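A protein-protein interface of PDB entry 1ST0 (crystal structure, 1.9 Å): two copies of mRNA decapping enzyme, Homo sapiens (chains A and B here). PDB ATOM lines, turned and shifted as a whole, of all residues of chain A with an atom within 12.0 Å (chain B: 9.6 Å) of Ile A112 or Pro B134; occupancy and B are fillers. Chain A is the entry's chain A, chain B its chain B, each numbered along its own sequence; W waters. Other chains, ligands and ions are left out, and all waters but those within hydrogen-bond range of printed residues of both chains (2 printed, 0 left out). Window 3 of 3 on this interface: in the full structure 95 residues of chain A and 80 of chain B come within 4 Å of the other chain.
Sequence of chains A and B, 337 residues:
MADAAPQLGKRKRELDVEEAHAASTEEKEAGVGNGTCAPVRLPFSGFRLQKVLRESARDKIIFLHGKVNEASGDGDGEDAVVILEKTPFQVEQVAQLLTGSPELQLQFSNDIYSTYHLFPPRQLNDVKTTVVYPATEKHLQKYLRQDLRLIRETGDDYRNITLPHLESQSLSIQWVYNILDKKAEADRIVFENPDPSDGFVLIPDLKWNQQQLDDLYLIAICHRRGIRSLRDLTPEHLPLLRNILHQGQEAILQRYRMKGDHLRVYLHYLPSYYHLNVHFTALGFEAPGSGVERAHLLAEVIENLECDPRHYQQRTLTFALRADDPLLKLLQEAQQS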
ATOM      1  N   LEU A 106     -10.604 -11.209  30.488  1.00  0.00           N
ATOM      2  CA  LEU A 106     -11.994 -11.639  30.403  1.00  0.00           C
ATOM      3  C   LEU A 106     -12.719 -11.030  31.590  1.00  0.00           C
ATOM      4  O   LEU A 106     -12.303 -11.281  32.739  1.00  0.00           O
ATOM      5  CB  LEU A 106     -12.078 -13.235  30.453  1.00  0.00           C
ATOM      6  CG  LEU A 106     -13.489 -13.846  30.480  1.00  0.00           C
ATOM      7  CD1 LEU A 106     -14.389 -13.454  29.258  1.00  0.00           C
ATOM      8  CD2 LEU A 106     -13.472 -15.441  30.538  1.00  0.00           C
ATOM      9  N   PHE A 108     -16.600 -11.047  31.789  1.00  0.00           N
ATOM     10  CA  PHE A 108     -17.840 -11.833  31.908  1.00  0.00           C
ATOM     11  C   PHE A 108     -17.843 -12.898  30.812  1.00  0.00           C
ATOM     12  O   PHE A 108     -17.369 -12.657  29.656  1.00  0.00           O
ATOM     13  CB  PHE A 108     -19.115 -11.034  31.635  1.00  0.00           C
ATOM     14  CG  PHE A 108     -19.281  -9.810  32.482  1.00  0.00           C
ATOM     15  CD1 PHE A 108     -19.613  -8.567  31.872  1.00  0.00           C
ATOM     16  CD2 PHE A 108     -19.190  -9.874  33.883  1.00  0.00           C
ATOM     17  CE1 PHE A 108     -19.785  -7.408  32.630  1.00  0.00           C
ATOM     18  CE2 PHE A 108     -19.354  -8.741  34.653  1.00  0.00           C
ATOM     19  CZ  PHE A 108     -19.663  -7.484  34.028  1.00  0.00           C
ATOM     20  N   SER A 109     -18.475 -14.032  31.090  1.00  0.00           N
ATOM     21  CA  SER A 109     -18.547 -15.049  30.069  1.00  0.00           C
ATOM     22  C   SER A 109     -19.739 -15.921  30.376  1.00  0.00           C
ATOM     23  O   SER A 109     -19.778 -16.570  31.438  1.00  0.00           O
ATOM     24  CB  SER A 109     -17.229 -15.871  30.066  1.00  0.00           C
ATOM     25  OG  SER A 109     -17.383 -17.157  29.494  1.00  0.00           O
ATOM     26  N   ASN A 110     -20.735 -15.902  29.499  1.00  0.00           N
ATOM     27  CA  ASN A 110     -21.800 -16.905  29.576  1.00  0.00           C
ATOM     28  C   ASN A 110     -22.345 -17.357  28.238  1.00  0.00           C
ATOM     29  O   ASN A 110     -23.030 -16.602  27.562  1.00  0.00           O
ATOM     30  CB  ASN A 110     -22.971 -16.493  30.494  1.00  0.00           C
ATOM     31  CG  ASN A 110     -23.645 -17.724  31.146  1.00  0.00           C
ATOM     32  OD1 ASN A 110     -24.122 -18.643  30.440  1.00  0.00           O
ATOM     33  ND2 ASN A 110     -23.608 -17.785  32.481  1.00  0.00           N
ATOM     34  N   ASP A 111     -22.073 -18.622  27.912  1.00  0.00           N
ATOM     35  CA  ASP A 111     -22.626 -19.254  26.724  1.00  0.00           C
ATOM     36  C   ASP A 111     -22.065 -18.448  25.522  1.00  0.00           C
ATOM     37  O   ASP A 111     -20.838 -18.323  25.391  1.00  0.00           O
ATOM     38  CB  ASP A 111     -24.162 -19.245  26.838  1.00  0.00           C
ATOM     39  CG  ASP A 111     -24.865 -20.157  25.805  1.00  0.00           C
ATOM     40  OD1 ASP A 111     -24.358 -21.265  25.514  1.00  0.00           O
ATOM     41  OD2 ASP A 111     -25.965 -19.843  25.260  1.00  0.00           O
ATOM     42  N   ILE A 112     -22.946 -17.849  24.725  1.00  0.00           N
ATOM     43  CA  ILE A 112     -22.560 -17.130  23.509  1.00  0.00           C
ATOM     44  C   ILE A 112     -22.130 -15.657  23.716  1.00  0.00           C
ATOM     45  O   ILE A 112     -21.671 -15.032  22.747  1.00  0.00           O
ATOM     46  CB  ILE A 112     -23.659 -17.213  22.427  1.00  0.00           C
ATOM     47  CG1 ILE A 112     -24.838 -16.300  22.764  1.00  0.00           C
ATOM     48  CG2 ILE A 112     -24.047 -18.714  22.109  1.00  0.00           C
ATOM     49  CD1 ILE A 112     -25.758 -16.060  21.549  1.00  0.00           C
ATOM     50  N   TYR A 113     -22.226 -15.166  24.965  1.00  0.00           N
ATOM     51  CA  TYR A 113     -21.920 -13.784  25.338  1.00  0.00           C
ATOM     52  C   TYR A 113     -20.697 -13.644  26.236  1.00  0.00           C
ATOM     53  O   TYR A 113     -20.546 -14.415  27.202  1.00  0.00           O
ATOM     54  CB  TYR A 113     -23.090 -13.187  26.111  1.00  0.00           C
ATOM     55  CG  TYR A 113     -24.418 -13.438  25.460  1.00  0.00           C
ATOM     56  CD1 TYR A 113     -25.291 -14.470  25.918  1.00  0.00           C
ATOM     57  CD2 TYR A 113     -24.828 -12.627  24.394  1.00  0.00           C
ATOM     58  CE1 TYR A 113     -26.534 -14.679  25.291  1.00  0.00           C
ATOM     59  CE2 TYR A 113     -26.036 -12.828  23.771  1.00  0.00           C
ATOM     60  CZ  TYR A 113     -26.896 -13.841  24.204  1.00  0.00           C
ATOM     61  OH  TYR A 113     -28.102 -13.981  23.506  1.00  0.00           O
ATOM     62  N   SER A 114     -19.817 -12.670  25.944  1.00  0.00           N
ATOM     63  CA  SER A 114     -18.633 -12.442  26.768  1.00  0.00           C
ATOM     64  C   SER A 114     -18.219 -10.986  26.648  1.00  0.00           C
ATOM     65  O   SER A 114     -18.518 -10.367  25.649  1.00  0.00           O
ATOM     66  CB  SER A 114     -17.457 -13.388  26.401  1.00  0.00           C
ATOM     67  OG  SER A 114     -17.265 -13.503  24.982  1.00  0.00           O
ATOM     68  N   THR A 115     -17.594 -10.452  27.694  1.00  0.00           N
ATOM     69  CA  THR A 115     -17.122  -9.081  27.761  1.00  0.00           C
ATOM     70  C   THR A 115     -15.675  -9.166  28.182  1.00  0.00           C
ATOM     71  O   THR A 115     -15.335  -9.892  29.161  1.00  0.00           O
ATOM     72  CB  THR A 115     -17.878  -8.317  28.777  1.00  0.00           C
ATOM     73  OG1 THR A 115     -19.282  -8.390  28.470  1.00  0.00           O
ATOM     74  CG2 THR A 115     -17.549  -6.772  28.722  1.00  0.00           C
ATOM     75  N   TYR A 116     -14.838  -8.431  27.463  1.00  0.00           N
ATOM     76  CA  TYR A 116     -13.439  -8.295  27.738  1.00  0.00           C
ATOM     77  C   TYR A 116     -13.035  -6.854  27.942  1.00  0.00           C
ATOM     78  O   TYR A 116     -13.776  -5.892  27.527  1.00  0.00           O
ATOM     79  CB  TYR A 116     -12.619  -8.817  26.541  1.00  0.00           C
ATOM     80  CG  TYR A 116     -12.915 -10.228  26.139  1.00  0.00           C
ATOM     81  CD1 TYR A 116     -14.076 -10.527  25.444  1.00  0.00           C
ATOM     82  CD2 TYR A 116     -12.009 -11.292  26.456  1.00  0.00           C
ATOM     83  CE1 TYR A 116     -14.377 -11.788  25.053  1.00  0.00           C
ATOM     84  CE2 TYR A 116     -12.330 -12.585  26.047  1.00  0.00           C
ATOM     85  CZ  TYR A 116     -13.520 -12.805  25.355  1.00  0.00           C
ATOM     86  OH  TYR A 116     -13.917 -14.036  24.945  1.00  0.00           O
ATOM     87  N   PRO B  43     -13.251 -15.878  21.571  1.00  0.00           N
ATOM     88  CA  PRO B  43     -13.710 -17.275  21.430  1.00  0.00           C
ATOM     89  C   PRO B  43     -13.656 -17.782  19.965  1.00  0.00           C
ATOM     90  O   PRO B  43     -14.234 -18.828  19.689  1.00  0.00           O
ATOM     91  CB  PRO B  43     -15.135 -17.249  21.980  1.00  0.00           C
ATOM     92  CG  PRO B  43     -15.611 -15.756  21.845  1.00  0.00           C
ATOM     93  CD  PRO B  43     -14.364 -14.918  21.718  1.00  0.00           C
ATOM     94  N   PHE B  44     -13.025 -17.039  19.048  1.00  0.00           N
ATOM     95  CA  PHE B  44     -12.881 -17.493  17.667  1.00  0.00           C
ATOM     96  C   PHE B  44     -11.508 -17.060  17.189  1.00  0.00           C
ATOM     97  O   PHE B  44     -10.840 -16.300  17.898  1.00  0.00           O
ATOM     98  CB  PHE B  44     -13.955 -16.865  16.779  1.00  0.00           C
ATOM     99  CG  PHE B  44     -14.104 -15.364  16.968  1.00  0.00           C
ATOM    100  CD1 PHE B  44     -13.221 -14.463  16.323  1.00  0.00           C
ATOM    101  CD2 PHE B  44     -15.117 -14.854  17.790  1.00  0.00           C
ATOM    102  CE1 PHE B  44     -13.350 -13.051  16.515  1.00  0.00           C
ATOM    103  CE2 PHE B  44     -15.269 -13.473  17.989  1.00  0.00           C
ATOM    104  CZ  PHE B  44     -14.395 -12.555  17.348  1.00  0.00           C
ATOM    105  N   HIS B  65     -20.433  -6.715  12.714  1.00  0.00           N
ATOM    106  CA  HIS B  65     -20.795  -8.084  12.323  1.00  0.00           C
ATOM    107  C   HIS B  65     -19.632  -8.572  11.564  1.00  0.00           C
ATOM    108  O   HIS B  65     -19.224  -8.001  10.531  1.00  0.00           O
ATOM    109  CB  HIS B  65     -22.032  -8.105  11.434  1.00  0.00           C
ATOM    110  CG  HIS B  65     -22.301  -9.434  10.771  1.00  0.00           C
ATOM    111  ND1 HIS B  65     -23.170  -9.558   9.699  1.00  0.00           N
ATOM    112  CD2 HIS B  65     -21.876 -10.699  11.052  1.00  0.00           C
ATOM    113  CE1 HIS B  65     -23.240 -10.829   9.332  1.00  0.00           C
ATOM    114  NE2 HIS B  65     -22.450 -11.540  10.122  1.00  0.00           N
ATOM    115  N   GLY B  66     -19.040  -9.622  12.070  1.00  0.00           N
ATOM    116  CA  GLY B  66     -17.939 -10.203  11.368  1.00  0.00           C
ATOM    117  C   GLY B  66     -18.217 -11.675  11.014  1.00  0.00           C
ATOM    118  O   GLY B  66     -19.095 -12.307  11.618  1.00  0.00           O
ATOM    119  N   VAL B  68     -16.103 -15.085  11.265  1.00  0.00           N
ATOM    120  CA  VAL B  68     -14.977 -15.585  11.995  1.00  0.00           C
ATOM    121  C   VAL B  68     -14.698 -17.043  11.594  1.00  0.00           C
ATOM    122  O   VAL B  68     -15.573 -17.702  11.006  1.00  0.00           O
ATOM    123  CB  VAL B  68     -15.248 -15.418  13.515  1.00  0.00           C
ATOM    124  CG1 VAL B  68     -15.555 -13.909  13.809  1.00  0.00           C
ATOM    125  CG2 VAL B  68     -16.416 -16.323  13.969  1.00  0.00           C
ATOM    126  N   ASN B  69     -13.489 -17.524  11.906  1.00  0.00           N
ATOM    127  CA  ASN B  69     -13.021 -18.903  11.574  1.00  0.00           C
ATOM    128  C   ASN B  69     -12.961 -19.243  10.067  1.00  0.00           C
ATOM    129  O   ASN B  69     -12.900 -20.412   9.699  1.00  0.00           O
ATOM    130  CB  ASN B  69     -13.820 -19.962  12.342  1.00  0.00           C
ATOM    131  CG  ASN B  69     -13.743 -19.773  13.867  1.00  0.00           C
ATOM    132  OD1 ASN B  69     -12.694 -19.412  14.420  1.00  0.00           O
ATOM    133  ND2 ASN B  69     -14.849 -20.030  14.546  1.00  0.00           N
ATOM    134  N   GLY B  77     -17.003 -19.870   7.434  1.00  0.00           N
ATOM    135  CA  GLY B  77     -17.160 -18.737   8.351  1.00  0.00           C
ATOM    136  C   GLY B  77     -18.418 -18.732   9.204  1.00  0.00           C
ATOM    137  O   GLY B  77     -19.498 -18.966   8.666  1.00  0.00           O
ATOM    138  N   GLU B  78     -18.281 -18.502  10.522  1.00  0.00           N
ATOM    139  CA  GLU B  78     -19.438 -18.325  11.437  1.00  0.00           C
ATOM    140  C   GLU B  78     -19.625 -16.828  11.752  1.00  0.00           C
ATOM    141  O   GLU B  78     -18.675 -16.047  11.599  1.00  0.00           O
ATOM    142  CB  GLU B  78     -19.267 -19.086  12.767  1.00  0.00           C
ATOM    143  CG  GLU B  78     -19.194 -20.595  12.626  1.00  0.00           C
ATOM    144  CD  GLU B  78     -18.699 -21.257  13.906  1.00  0.00           C
ATOM    145  OE1 GLU B  78     -19.530 -21.791  14.664  1.00  0.00           O
ATOM    146  OE2 GLU B  78     -17.471 -21.227  14.176  1.00  0.00           O
ATOM    147  N   ASP B  79     -20.833 -16.462  12.183  1.00  0.00           N
ATOM    148  CA  ASP B  79     -21.185 -15.067  12.441  1.00  0.00           C
ATOM    149  C   ASP B  79     -20.847 -14.696  13.882  1.00  0.00           C
ATOM    150  O   ASP B  79     -21.079 -15.484  14.802  1.00  0.00           O
ATOM    151  CB  ASP B  79     -22.676 -14.827  12.196  1.00  0.00           C
ATOM    152  CG  ASP B  79     -23.051 -14.890  10.713  1.00  0.00           C
ATOM    153  OD1 ASP B  79     -22.334 -14.291   9.864  1.00  0.00           O
ATOM    154  OD2 ASP B  79     -24.052 -15.516  10.303  1.00  0.00           O
ATOM    155  N   ALA B  80     -20.322 -13.487  14.064  1.00  0.00           N
ATOM    156  CA  ALA B  80     -20.080 -12.925  15.405  1.00  0.00           C
ATOM    157  C   ALA B  80     -20.492 -11.466  15.431  1.00  0.00           C
ATOM    158  O   ALA B  80     -20.380 -10.728  14.379  1.00  0.00           O
ATOM    159  CB  ALA B  80     -18.615 -13.040  15.775  1.00  0.00           C
ATOM    160  N   VAL B  81     -20.982 -11.028  16.597  1.00  0.00           N
ATOM    161  CA  VAL B  81     -21.131  -9.581  16.809  1.00  0.00           C
ATOM    162  C   VAL B  81     -20.056  -9.192  17.809  1.00  0.00           C
ATOM    163  O   VAL B  81     -19.856  -9.909  18.804  1.00  0.00           O
ATOM    164  CB  VAL B  81     -22.518  -9.246  17.308  1.00  0.00           C
ATOM    165  CG1 VAL B  81     -22.578  -7.753  17.804  1.00  0.00           C
ATOM    166  CG2 VAL B  81     -23.529  -9.547  16.215  1.00  0.00           C
ATOM    167  N   VAL B  82     -19.314  -8.107  17.539  1.00  0.00           N
ATOM    168  CA  VAL B  82     -18.351  -7.544  18.498  1.00  0.00           C
ATOM    169  C   VAL B  82     -18.728  -6.092  18.638  1.00  0.00           C
ATOM    170  O   VAL B  82     -18.822  -5.388  17.603  1.00  0.00           O
ATOM    171  CB  VAL B  82     -16.951  -7.597  18.023  1.00  0.00           C
ATOM    172  CG1 VAL B  82     -15.927  -7.147  19.092  1.00  0.00           C
ATOM    173  CG2 VAL B  82     -16.623  -8.994  17.562  1.00  0.00           C
ATOM    174  N   THR B 130     -17.576  -6.400  23.764  1.00  0.00           N
ATOM    175  CA  THR B 130     -18.609  -7.386  23.986  1.00  0.00           C
ATOM    176  C   THR B 130     -18.718  -8.263  22.748  1.00  0.00           C
ATOM    177  O   THR B 130     -18.819  -7.736  21.628  1.00  0.00           O
ATOM    178  CB  THR B 130     -19.892  -6.695  24.307  1.00  0.00           C
ATOM    179  OG1 THR B 130     -19.713  -5.930  25.506  1.00  0.00           O
ATOM    180  CG2 THR B 130     -21.033  -7.675  24.612  1.00  0.00           C
ATOM    181  N   VAL B 131     -18.654  -9.593  22.947  1.00  0.00           N
ATOM    182  CA  VAL B 131     -18.761 -10.601  21.890  1.00  0.00           C
ATOM    183  C   VAL B 131     -20.015 -11.436  22.022  1.00  0.00           C
ATOM    184  O   VAL B 131     -20.344 -11.929  23.123  1.00  0.00           O
ATOM    185  CB  VAL B 131     -17.516 -11.525  21.908  1.00  0.00           C
ATOM    186  CG1 VAL B 131     -17.539 -12.565  20.755  1.00  0.00           C
ATOM    187  CG2 VAL B 131     -16.244 -10.646  21.863  1.00  0.00           C
ATOM    188  N   VAL B 132     -20.738 -11.528  20.908  1.00  0.00           N
ATOM    189  CA  VAL B 132     -21.798 -12.489  20.706  1.00  0.00           C
ATOM    190  C   VAL B 132     -21.270 -13.476  19.654  1.00  0.00           C
ATOM    191  O   VAL B 132     -21.037 -13.089  18.489  1.00  0.00           O
ATOM    192  CB  VAL B 132     -23.113 -11.850  20.220  1.00  0.00           C
ATOM    193  CG1 VAL B 132     -24.143 -12.923  20.066  1.00  0.00           C
ATOM    194  CG2 VAL B 132     -23.627 -10.757  21.185  1.00  0.00           C
ATOM    195  N   TYR B 133     -21.074 -14.747  20.062  1.00  0.00           N
ATOM    196  CA  TYR B 133     -20.507 -15.772  19.180  1.00  0.00           C
ATOM    197  C   TYR B 133     -20.963 -17.205  19.587  1.00  0.00           C
ATOM    198  O   TYR B 133     -20.800 -17.565  20.730  1.00  0.00           O
ATOM    199  CB  TYR B 133     -18.971 -15.793  19.210  1.00  0.00           C
ATOM    200  CG  TYR B 133     -18.454 -17.105  18.580  1.00  0.00           C
ATOM    201  CD1 TYR B 133     -18.431 -17.269  17.190  1.00  0.00           C
ATOM    202  CD2 TYR B 133     -18.053 -18.189  19.377  1.00  0.00           C
ATOM    203  CE1 TYR B 133     -18.030 -18.473  16.609  1.00  0.00           C
ATOM    204  CE2 TYR B 133     -17.635 -19.406  18.809  1.00  0.00           C
ATOM    205  CZ  TYR B 133     -17.618 -19.542  17.436  1.00  0.00           C
ATOM    206  OH  TYR B 133     -17.200 -20.732  16.862  1.00  0.00           O
ATOM    207  N   PRO B 134     -21.520 -18.016  18.675  1.00  0.00           N
ATOM    208  CA  PRO B 134     -21.960 -17.610  17.323  1.00  0.00           C
ATOM    209  C   PRO B 134     -23.140 -16.621  17.358  1.00  0.00           C
ATOM    210  O   PRO B 134     -24.003 -16.760  18.205  1.00  0.00           O
ATOM    211  CB  PRO B 134     -22.452 -18.951  16.696  1.00  0.00           C
ATOM    212  CG  PRO B 134     -21.883 -20.032  17.578  1.00  0.00           C
ATOM    213  CD  PRO B 134     -21.782 -19.455  18.951  1.00  0.00           C
ATOM    214  N   ALA B 135     -23.195 -15.656  16.434  1.00  0.00           N
ATOM    215  CA  ALA B 135     -24.334 -14.767  16.389  1.00  0.00           C
ATOM    216  C   ALA B 135     -25.448 -15.286  15.467  1.00  0.00           C
ATOM    217  O   ALA B 135     -25.170 -15.752  14.369  1.00  0.00           O
ATOM    218  CB  ALA B 135     -23.890 -13.381  15.919  1.00  0.00           C
ATOM    219  N   THR B 136     -26.698 -15.160  15.889  1.00  0.00           N
ATOM    220  CA  THR B 136     -27.800 -15.495  14.997  1.00  0.00           C
ATOM    221  C   THR B 136     -28.255 -14.308  14.178  1.00  0.00           C
ATOM    222  O   THR B 136     -27.903 -13.148  14.471  1.00  0.00           O
ATOM    223  CB  THR B 136     -29.019 -16.026  15.765  1.00  0.00           C
ATOM    224  OG1 THR B 136     -29.621 -14.946  16.508  1.00  0.00           O
ATOM    225  CG2 THR B 136     -28.607 -17.108  16.792  1.00  0.00           C
ATOM    226  N   GLU B 137     -29.075 -14.609  13.163  1.00  0.00           N
ATOM    227  CA  GLU B 137     -29.726 -13.578  12.367  1.00  0.00           C
ATOM    228  C   GLU B 137     -30.576 -12.639  13.218  1.00  0.00           C
ATOM    229  O   GLU B 137     -30.693 -11.455  12.931  1.00  0.00           O
ATOM    230  CB  GLU B 137     -30.569 -14.208  11.250  1.00  0.00           C
ATOM    231  CG  GLU B 137     -31.300 -13.197  10.373  1.00  0.00           C
ATOM    232  CD  GLU B 137     -30.373 -12.214   9.654  1.00  0.00           C
ATOM    233  OE1 GLU B 137     -30.854 -11.082   9.411  1.00  0.00           O
ATOM    234  OE2 GLU B 137     -29.186 -12.534   9.325  1.00  0.00           O
ATOM    235  N   LYS B 138     -31.134 -13.161  14.288  1.00  0.00           N
ATOM    236  CA  LYS B 138     -31.842 -12.345  15.267  1.00  0.00           C
ATOM    237  C   LYS B 138     -30.914 -11.362  16.030  1.00  0.00           C
ATOM    238  O   LYS B 138     -31.358 -10.272  16.450  1.00  0.00           O
ATOM    239  CB  LYS B 138     -32.562 -13.286  16.228  1.00  0.00           C
ATOM    240  CG  LYS B 138     -33.597 -12.674  17.176  1.00  0.00           C
ATOM    241  CD  LYS B 138     -34.386 -13.800  17.938  1.00  0.00           C
ATOM    242  CE  LYS B 138     -35.864 -13.920  17.484  1.00  0.00           C
ATOM    243  NZ  LYS B 138     -36.565 -15.163  18.029  1.00  0.00           N
ATOM    244  N   HIS B 139     -29.652 -11.723  16.252  1.00  0.00           N
ATOM    245  CA  HIS B 139     -28.734 -10.761  16.896  1.00  0.00           C
ATOM    246  C   HIS B 139     -28.400  -9.653  15.905  1.00  0.00           C
ATOM    247  O   HIS B 139     -28.274  -8.493  16.272  1.00  0.00           O
ATOM    248  CB  HIS B 139     -27.427 -11.425  17.314  1.00  0.00           C
ATOM    249  CG  HIS B 139     -27.572 -12.367  18.469  1.00  0.00           C
ATOM    250  ND1 HIS B 139     -27.341 -13.723  18.350  1.00  0.00           N
ATOM    251  CD2 HIS B 139     -27.942 -12.154  19.756  1.00  0.00           C
ATOM    252  CE1 HIS B 139     -27.544 -14.299  19.522  1.00  0.00           C
ATOM    253  NE2 HIS B 139     -27.901 -13.368  20.395  1.00  0.00           N
ATOM    254  N   LEU B 140     -28.233 -10.034  14.646  1.00  0.00           N
ATOM    255  CA  LEU B 140     -27.851  -9.082  13.610  1.00  0.00           C
ATOM    256  C   LEU B 140     -28.943  -8.062  13.506  1.00  0.00           C
ATOM    257  O   LEU B 140     -28.690  -6.847  13.440  1.00  0.00           O
ATOM    258  CB  LEU B 140     -27.658  -9.778  12.289  1.00  0.00           C
ATOM    259  CG  LEU B 140     -26.519 -10.769  12.312  1.00  0.00           C
ATOM    260  CD1 LEU B 140     -26.343 -11.307  10.912  1.00  0.00           C
ATOM    261  CD2 LEU B 140     -25.233 -10.138  12.860  1.00  0.00           C
ATOM    262  N   TYR B 143     -29.124  -5.210  16.303  1.00  0.00           N
ATOM    263  CA  TYR B 143     -28.185  -4.091  16.338  1.00  0.00           C
ATOM    264  C   TYR B 143     -28.175  -3.227  15.065  1.00  0.00           C
ATOM    265  O   TYR B 143     -27.724  -2.058  15.104  1.00  0.00           O
ATOM    266  CB  TYR B 143     -26.778  -4.587  16.679  1.00  0.00           C
ATOM    267  CG  TYR B 143     -26.708  -5.283  18.056  1.00  0.00           C
ATOM    268  CD1 TYR B 143     -26.447  -6.637  18.150  1.00  0.00           C
ATOM    269  CD2 TYR B 143     -26.897  -4.574  19.236  1.00  0.00           C
ATOM    270  CE1 TYR B 143     -26.367  -7.281  19.369  1.00  0.00           C
ATOM    271  CE2 TYR B 143     -26.817  -5.217  20.483  1.00  0.00           C
ATOM    272  CZ  TYR B 143     -26.560  -6.576  20.519  1.00  0.00           C
ATOM    273  OH  TYR B 143     -26.482  -7.239  21.711  1.00  0.00           O
HETATM  274  O   HOH W   1     -18.732 -14.832  23.274  1.00  0.00           O
HETATM  275  O   HOH W   2     -20.962  -6.014  27.734  1.00  0.00           O
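O of Ile A112 lies close to O of Val B131, at 3.4 Å. NE2 of His B139 lies within hydrogen-bond range of OH of Tyr A113 (3.2 Å). The backbone carbonyl oxygen of Ile A112 lies within hydrogen-bond range of the backbone NH of Tyr B133. N of Val B131 lies within hydrogen-bond range of O of Ser A114, at 2.8 Å.
The backbone NH of Thr A115 lies within hydrogen-bond range of the backbone carbonyl oxygen of Phe A108 (3.0 Å). The backbone carbonyl oxygen of Val B81 sits at hydrogen-bond distance from the backbone NH of Val B132 (2.8 Å). OG of Ser A114 sits close to OH of Tyr A116. ND2 of Asn B69 sits at hydrogen-bond distance from OH of Tyr B133 (3.4 Å). A ring nitrogen (ND1) of His B139 sits at hydrogen-bond distance from the backbone NH of Thr B136 (2.9 Å). The side-chain hydroxyl (OH) of Tyr B133 sits at hydrogen-bond distance from the side-chain carboxylate (OE2) of Glu B78 (2.7 Å).
Among the printed residues, pairs that only touch across the chains: Ile A112 with His B139 (3.2 Å), Ile A112 with Val B132 (3.3 Å), Tyr A113 with Val B131 (3.3 Å), Tyr A116 with Pro B43 (3.4 Å), Ser A114 with Thr B130 (3.4 Å), Ile A112 with Pro B134 (3.8 Å), Tyr A116 with Val B131 (3.9 Å), Thr A115 with Thr B130 (3.9 Å) and Tyr A113 with Val B132 (3.9 Å).
Leu A106 touches none of the printed residues of chain B. Phe A108 touches none of the printed residues of chain B. No residue of chain B comes within 4 Å of Asp A111. Of chain B, only Val B131 (3.3 Å), Val B132 (3.9 Å) and His B139 (3.2 Å) come within 4 Å of Tyr A113. Printed residues of chain B within 4 Å of Ser A114: Thr B130 and Val B131. Printed residues of chain B within 4 Å of Thr A115: Thr B130. Printed residues of chain B within 4 Å of Tyr A116: Pro B43 (3.4 Å) and Val B131 (3.9 Å). Printed residues of chain A within 4 Å of Pro B43: Tyr A116 (3.4 Å). No residue of chain A comes within 4 Å of Glu B78. No residue of chain A comes within 4 Å of Asp B79. No residue of chain A comes within 4 Å of Ala B80. Of chain A, only Ile A112, Tyr A113, Ser A114 and Tyr A116 come within 4 Å of Val B131. Val B132 touches two residues of chain A. Of chain A, only Ile A112 (3.8 Å) comes within 4 Å of Pro B134. No residue of chain A comes within 4 Å of Ala B135. Printed residues of chain A within 4 Å of His B139: Ile A112 and Tyr A113. The nearest printed residue of chain B that does not touch Tyr A116 is Thr B130 (5.0 Å).
Of the 10 printed residues of chain A, 5 touch a printed residue of chain B. Hydrophobic or aromatic side chains of chain A within 4 Å of the printed part of chain B: Ile A112, Tyr A113 and Tyr A116. Along chain A the printed residues that touch a printed residue of chain B span positions 112 to 116. Hydrophobic or aromatic side chains of chain B that line the printed part of chain A: Pro B43, Val B131, Val B132, Pro B134 and His B139. Along chain B the printed residues that touch a printed residue of chain A span positions 43 to 139. Among the printed residues, no Asp or Glu carboxylate lies within 4 Å of a Lys or Arg side-chain nitrogen of the other chain.
No position is printed for both chains. Of the 13 pairs that touch across the chains among the printed residues, none has its exchanged pair printed and touching as well.
Water W2 lies within hydrogen-bond range of OG1 of Thr B130 (2.6 Å) and OG1 of Thr A115 (3.0 Å). Water W1 lies within hydrogen-bond range of the side-chain hydroxyl (OG) of Ser A114 (2.6 Å), the backbone carbonyl oxygen (O) of Ile A112 (3.0 Å) and the backbone carbonyl oxygen (O) of Val B131 (3.3 Å).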
